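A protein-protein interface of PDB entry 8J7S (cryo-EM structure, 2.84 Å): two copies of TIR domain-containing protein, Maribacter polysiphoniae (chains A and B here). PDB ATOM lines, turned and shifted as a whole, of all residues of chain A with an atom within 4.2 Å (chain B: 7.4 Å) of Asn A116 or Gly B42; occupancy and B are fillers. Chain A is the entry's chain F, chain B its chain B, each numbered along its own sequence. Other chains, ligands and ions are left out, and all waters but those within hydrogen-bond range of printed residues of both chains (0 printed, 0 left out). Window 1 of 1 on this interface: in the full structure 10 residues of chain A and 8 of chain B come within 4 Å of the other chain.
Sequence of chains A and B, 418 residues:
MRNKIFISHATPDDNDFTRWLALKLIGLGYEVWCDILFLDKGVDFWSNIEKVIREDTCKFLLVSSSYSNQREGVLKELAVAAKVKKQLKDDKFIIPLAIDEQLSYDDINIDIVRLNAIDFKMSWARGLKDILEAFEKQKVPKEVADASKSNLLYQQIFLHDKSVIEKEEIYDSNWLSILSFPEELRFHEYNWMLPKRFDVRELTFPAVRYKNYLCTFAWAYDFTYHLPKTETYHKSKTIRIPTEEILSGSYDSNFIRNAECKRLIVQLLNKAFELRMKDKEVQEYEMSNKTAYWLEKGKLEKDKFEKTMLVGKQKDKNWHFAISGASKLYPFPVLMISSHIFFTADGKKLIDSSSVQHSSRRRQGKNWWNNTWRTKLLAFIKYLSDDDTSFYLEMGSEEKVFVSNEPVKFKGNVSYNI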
ATOM      1  N   ASP A  91     -29.178  -9.873 -27.967  1.00  0.00           N
ATOM      2  CA  ASP A  91     -27.836  -9.619 -27.455  1.00  0.00           C
ATOM      3  C   ASP A  91     -27.651 -10.170 -26.047  1.00  0.00           C
ATOM      4  O   ASP A  91     -26.540 -10.569 -25.681  1.00  0.00           O
ATOM      5  CB  ASP A  91     -27.551  -8.118 -27.481  1.00  0.00           C
ATOM      6  CG  ASP A  91     -26.108  -7.790 -27.162  1.00  0.00           C
ATOM      7  OD1 ASP A  91     -25.247  -8.688 -27.268  1.00  0.00           O
ATOM      8  OD2 ASP A  91     -25.835  -6.624 -26.810  1.00  0.00           O
ATOM      9  N   LYS A  92     -28.719 -10.212 -25.251  1.00  0.00           N
ATOM     10  CA  LYS A  92     -28.645 -10.610 -23.851  1.00  0.00           C
ATOM     11  C   LYS A  92     -28.994 -12.080 -23.646  1.00  0.00           C
ATOM     12  O   LYS A  92     -29.578 -12.442 -22.619  1.00  0.00           O
ATOM     13  CB  LYS A  92     -29.555  -9.719 -23.006  1.00  0.00           C
ATOM     14  CG  LYS A  92     -28.964  -8.355 -22.693  1.00  0.00           C
ATOM     15  CD  LYS A  92     -29.833  -7.228 -23.222  1.00  0.00           C
ATOM     16  CE  LYS A  92     -31.306  -7.499 -22.979  1.00  0.00           C
ATOM     17  NZ  LYS A  92     -32.156  -6.358 -23.412  1.00  0.00           N
ATOM     18  N   ARG A 114     -16.307 -10.788 -23.880  1.00  0.00           N
ATOM     19  CA  ARG A 114     -16.922  -9.496 -24.149  1.00  0.00           C
ATOM     20  C   ARG A 114     -18.200  -9.264 -23.357  1.00  0.00           C
ATOM     21  O   ARG A 114     -18.714  -8.142 -23.371  1.00  0.00           O
ATOM     22  CB  ARG A 114     -17.225  -9.369 -25.642  1.00  0.00           C
ATOM     23  CG  ARG A 114     -16.041  -9.620 -26.563  1.00  0.00           C
ATOM     24  CD  ARG A 114     -15.250  -8.353 -26.807  1.00  0.00           C
ATOM     25  NE  ARG A 114     -16.059  -7.323 -27.445  1.00  0.00           N
ATOM     26  CZ  ARG A 114     -15.618  -6.111 -27.753  1.00  0.00           C
ATOM     27  NH1 ARG A 114     -14.364  -5.755 -27.528  1.00  0.00           N
ATOM     28  NH2 ARG A 114     -16.457  -5.235 -28.297  1.00  0.00           N
ATOM     29  N   LEU A 115     -18.722 -10.275 -22.673  1.00  0.00           N
ATOM     30  CA  LEU A 115     -20.020 -10.165 -22.027  1.00  0.00           C
ATOM     31  C   LEU A 115     -19.895  -9.649 -20.595  1.00  0.00           C
ATOM     32  O   LEU A 115     -18.832  -9.707 -19.972  1.00  0.00           O
ATOM     33  CB  LEU A 115     -20.740 -11.512 -22.038  1.00  0.00           C
ATOM     34  CG  LEU A 115     -21.191 -12.008 -23.412  1.00  0.00           C
ATOM     35  CD1 LEU A 115     -21.890 -13.343 -23.290  1.00  0.00           C
ATOM     36  CD2 LEU A 115     -22.102 -10.992 -24.081  1.00  0.00           C
ATOM     37  N   ASN A 116     -21.013  -9.142 -20.082  1.00  0.00           N
ATOM     38  CA  ASN A 116     -21.102  -8.574 -18.741  1.00  0.00           C
ATOM     39  C   ASN A 116     -21.676  -9.636 -17.806  1.00  0.00           C
ATOM     40  O   ASN A 116     -22.866  -9.956 -17.875  1.00  0.00           O
ATOM     41  CB  ASN A 116     -21.971  -7.318 -18.755  1.00  0.00           C
ATOM     42  CG  ASN A 116     -21.894  -6.537 -17.465  1.00  0.00           C
ATOM     43  OD1 ASN A 116     -20.873  -6.545 -16.777  1.00  0.00           O
ATOM     44  ND2 ASN A 116     -22.977  -5.845 -17.131  1.00  0.00           N
ATOM     45  N   ALA A 117     -20.831 -10.174 -16.935  1.00  0.00           N
ATOM     46  CA  ALA A 117     -21.197 -11.300 -16.091  1.00  0.00           C
ATOM     47  C   ALA A 117     -21.799 -10.837 -14.767  1.00  0.00           C
ATOM     48  O   ALA A 117     -21.687  -9.674 -14.372  1.00  0.00           O
ATOM     49  CB  ALA A 117     -19.979 -12.183 -15.826  1.00  0.00           C
ATOM     50  N   ASP B  35     -23.170   2.954 -15.893  1.00  0.00           N
ATOM     51  CA  ASP B  35     -23.065   1.500 -15.957  1.00  0.00           C
ATOM     52  C   ASP B  35     -23.676   0.845 -14.725  1.00  0.00           C
ATOM     53  O   ASP B  35     -24.364  -0.178 -14.833  1.00  0.00           O
ATOM     54  CB  ASP B  35     -21.604   1.086 -16.116  1.00  0.00           C
ATOM     55  CG  ASP B  35     -20.691   1.792 -15.142  1.00  0.00           C
ATOM     56  OD1 ASP B  35     -21.165   2.712 -14.445  1.00  0.00           O
ATOM     57  OD2 ASP B  35     -19.500   1.426 -15.069  1.00  0.00           O
ATOM     58  N   PHE B  38     -27.712   1.123 -15.374  1.00  0.00           N
ATOM     59  CA  PHE B  38     -28.415   0.792 -16.606  1.00  0.00           C
ATOM     60  C   PHE B  38     -27.697  -0.209 -17.498  1.00  0.00           C
ATOM     61  O   PHE B  38     -28.327  -0.732 -18.424  1.00  0.00           O
ATOM     62  CB  PHE B  38     -28.697   2.067 -17.416  1.00  0.00           C
ATOM     63  CG  PHE B  38     -29.720   2.966 -16.787  1.00  0.00           C
ATOM     64  CD1 PHE B  38     -31.070   2.767 -17.014  1.00  0.00           C
ATOM     65  CD2 PHE B  38     -29.332   4.005 -15.960  1.00  0.00           C
ATOM     66  CE1 PHE B  38     -32.014   3.590 -16.433  1.00  0.00           C
ATOM     67  CE2 PHE B  38     -30.272   4.832 -15.376  1.00  0.00           C
ATOM     68  CZ  PHE B  38     -31.615   4.623 -15.614  1.00  0.00           C
ATOM     69  N   LEU B  39     -26.421  -0.497 -17.261  1.00  0.00           N
ATOM     70  CA  LEU B  39     -25.729  -1.506 -18.051  1.00  0.00           C
ATOM     71  C   LEU B  39     -26.310  -2.883 -17.754  1.00  0.00           C
ATOM     72  O   LEU B  39     -26.494  -3.254 -16.590  1.00  0.00           O
ATOM     73  CB  LEU B  39     -24.231  -1.479 -17.749  1.00  0.00           C
ATOM     74  CG  LEU B  39     -23.360  -2.528 -18.440  1.00  0.00           C
ATOM     75  CD1 LEU B  39     -23.269  -2.249 -19.929  1.00  0.00           C
ATOM     76  CD2 LEU B  39     -21.974  -2.575 -17.813  1.00  0.00           C
ATOM     77  N   ASP B  40     -26.598  -3.643 -18.808  1.00  0.00           N
ATOM     78  CA  ASP B  40     -27.264  -4.926 -18.668  1.00  0.00           C
ATOM     79  C   ASP B  40     -26.243  -6.039 -18.440  1.00  0.00           C
ATOM     80  O   ASP B  40     -25.031  -5.817 -18.410  1.00  0.00           O
ATOM     81  CB  ASP B  40     -28.127  -5.213 -19.895  1.00  0.00           C
ATOM     82  CG  ASP B  40     -29.506  -4.597 -19.792  1.00  0.00           C
ATOM     83  OD1 ASP B  40     -30.383  -5.205 -19.147  1.00  0.00           O
ATOM     84  OD2 ASP B  40     -29.716  -3.503 -20.356  1.00  0.00           O
ATOM     85  N   LYS B  41     -26.746  -7.261 -18.278  1.00  0.00           N
ATOM     86  CA  LYS B  41     -25.923  -8.412 -17.915  1.00  0.00           C
ATOM     87  C   LYS B  41     -25.652  -9.220 -19.179  1.00  0.00           C
ATOM     88  O   LYS B  41     -26.355 -10.178 -19.500  1.00  0.00           O
ATOM     89  CB  LYS B  41     -26.608  -9.231 -16.831  1.00  0.00           C
ATOM     90  CG  LYS B  41     -27.235  -8.366 -15.753  1.00  0.00           C
ATOM     91  CD  LYS B  41     -26.412  -8.377 -14.480  1.00  0.00           C
ATOM     92  CE  LYS B  41     -25.546  -7.139 -14.366  1.00  0.00           C
ATOM     93  NZ  LYS B  41     -24.681  -7.181 -13.159  1.00  0.00           N
ATOM     94  N   GLY B  42     -24.628  -8.795 -19.909  1.00  0.00           N
ATOM     95  CA  GLY B  42     -24.168  -9.412 -21.137  1.00  0.00           C
ATOM     96  C   GLY B  42     -24.714  -8.635 -22.312  1.00  0.00           C
ATOM     97  O   GLY B  42     -25.821  -8.908 -22.783  1.00  0.00           O
ATOM     98  N   VAL B  43     -23.947  -7.661 -22.791  1.00  0.00           N
ATOM     99  CA  VAL B  43     -24.391  -6.821 -23.896  1.00  0.00           C
ATOM    100  C   VAL B  43     -23.256  -6.550 -24.873  1.00  0.00           C
ATOM    101  O   VAL B  43     -23.413  -5.743 -25.798  1.00  0.00           O
ATOM    102  CB  VAL B  43     -24.992  -5.504 -23.378  1.00  0.00           C
ATOM    103  CG1 VAL B  43     -26.462  -5.689 -23.061  1.00  0.00           C
ATOM    104  CG2 VAL B  43     -24.240  -5.031 -22.148  1.00  0.00           C
ATOM    105  N   ASP B  44     -22.104  -7.193 -24.668  1.00  0.00           N
ATOM    106  CA  ASP B  44     -20.844  -6.739 -25.257  1.00  0.00           C
ATOM    107  C   ASP B  44     -20.563  -5.305 -24.797  1.00  0.00           C
ATOM    108  O   ASP B  44     -20.548  -4.353 -25.579  1.00  0.00           O
ATOM    109  CB  ASP B  44     -20.871  -6.848 -26.788  1.00  0.00           C
ATOM    110  CG  ASP B  44     -19.497  -7.061 -27.388  1.00  0.00           C
ATOM    111  OD1 ASP B  44     -18.727  -6.082 -27.482  1.00  0.00           O
ATOM    112  OD2 ASP B  44     -19.195  -8.203 -27.789  1.00  0.00           O
ATOM    113  N   PHE B  45     -20.349  -5.190 -23.482  1.00  0.00           N
ATOM    114  CA  PHE B  45     -20.569  -3.923 -22.785  1.00  0.00           C
ATOM    115  C   PHE B  45     -19.729  -2.789 -23.361  1.00  0.00           C
ATOM    116  O   PHE B  45     -20.175  -1.638 -23.386  1.00  0.00           O
ATOM    117  CB  PHE B  45     -20.308  -4.092 -21.284  1.00  0.00           C
ATOM    118  CG  PHE B  45     -18.915  -4.544 -20.945  1.00  0.00           C
ATOM    119  CD1 PHE B  45     -17.891  -3.627 -20.780  1.00  0.00           C
ATOM    120  CD2 PHE B  45     -18.634  -5.887 -20.770  1.00  0.00           C
ATOM    121  CE1 PHE B  45     -16.614  -4.043 -20.460  1.00  0.00           C
ATOM    122  CE2 PHE B  45     -17.358  -6.308 -20.451  1.00  0.00           C
ATOM    123  CZ  PHE B  45     -16.348  -5.385 -20.296  1.00  0.00           C
ATOM    124  N   ASN B  48     -21.617  -1.610 -26.182  1.00  0.00           N
ATOM    125  CA  ASN B  48     -22.847  -0.972 -25.723  1.00  0.00           C
ATOM    126  C   ASN B  48     -22.588   0.461 -25.270  1.00  0.00           C
ATOM    127  O   ASN B  48     -23.319   1.385 -25.644  1.00  0.00           O
ATOM    128  CB  ASN B  48     -23.469  -1.791 -24.593  1.00  0.00           C
ATOM    129  CG  ASN B  48     -24.900  -1.394 -24.311  1.00  0.00           C
ATOM    130  OD1 ASN B  48     -25.580  -0.829 -25.166  1.00  0.00           O
ATOM    131  ND2 ASN B  48     -25.366  -1.685 -23.103  1.00  0.00           N
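The backbone carbonyl oxygen (O) of Asp B40 is in hydrogen-bond range of the side-chain amide nitrogen (ND2) of Asn A116, 2.4 Å away.
The backbone NH of Gly B42 is in hydrogen-bond range of the backbone carbonyl oxygen of Asn A116 (2.9 Å).
NH2 of Arg A114 is in salt-bridge range of OD1 of Asp B44 (2.6 Å).
The backbone carbonyl oxygen of Arg A114 sits at hydrogen-bond distance from the backbone NH of Phe B45.
The backbone carbonyl oxygen of Asp A91 lies close to the backbone carbonyl oxygen of Gly B42 (3.4 Å).
O of Val B43 lies close to OD2 of Asp A91 (2.8 Å).
Printed residues of chain B within 4 Å of Asp A91: Gly B42 (3.4 Å) and Val B43 (2.8 Å).
Of the printed residues of chain B, Leu A115 touches Gly B42, Asp B44 and Phe B45.
Of chain B, only Leu B39 (3.5 Å), Asp B40 (2.4 Å), Lys B41 (3.2 Å) and Gly B42 (2.9 Å) come within 4 Å of Asn A116.
Ala A117 touches none of the printed residues of chain B.
Phe B38 touches none of the printed residues of chain A.
Printed residues of chain A within 4 Å of Lys B41: Asn A116 (3.2 Å).
Gly B42 touches just these residues of chain A: Asp A91 (3.4 Å), Lys A92 (3.2 Å), Leu A115 (3.9 Å) and Asn A116 (2.9 Å).
Printed residues of chain A within 4 Å of Val B43: Asp A91 (2.8 Å) and Lys A92 (3.7 Å).
Printed residues of chain A within 4 Å of Asp B44: Arg A114 and Leu A115.
The nearest printed residue of chain A that does not touch Gly B42 is Ala A117 (5.0 Å).
Of the 10 printed residues of chain B, 7 touch a printed residue of chain A.
Printed residues of chain B that touch a printed residue of chain A: Leu B39, Asp B40, Lys B41, Gly B42, Val B43, Asp B44 and Phe B45.
Hydrophobic or aromatic side chains of chain B within 4 Å of the printed part of chain A: Leu B39, Val B43 and Phe B45.
Among the printed residues, 13 pairs touch across the chains.
Among the printed residues, Asp or Glu carboxylates within 4 Å of a Lys or Arg side-chain nitrogen of the other chain: Arg A114 with Asp B44.
No position is printed for both chains.
Of the 13 pairs that touch across the chains among the printed residues, none has its exchanged pair printed and touching as well.
Among the printed residues, pairs that only touch across the chains: Asn A116 with Lys B41 (3.2 Å), Lys A92 with Gly B42 (3.2 Å), Asn A116 with Leu B39 (3.5 Å), Lys A92 with Val B43 (3.7 Å), Leu A115 with Phe B45 (3.7 Å), Leu A115 with Asp B44 (3.8 Å) and Leu A115 with Gly B42 (3.9 Å).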
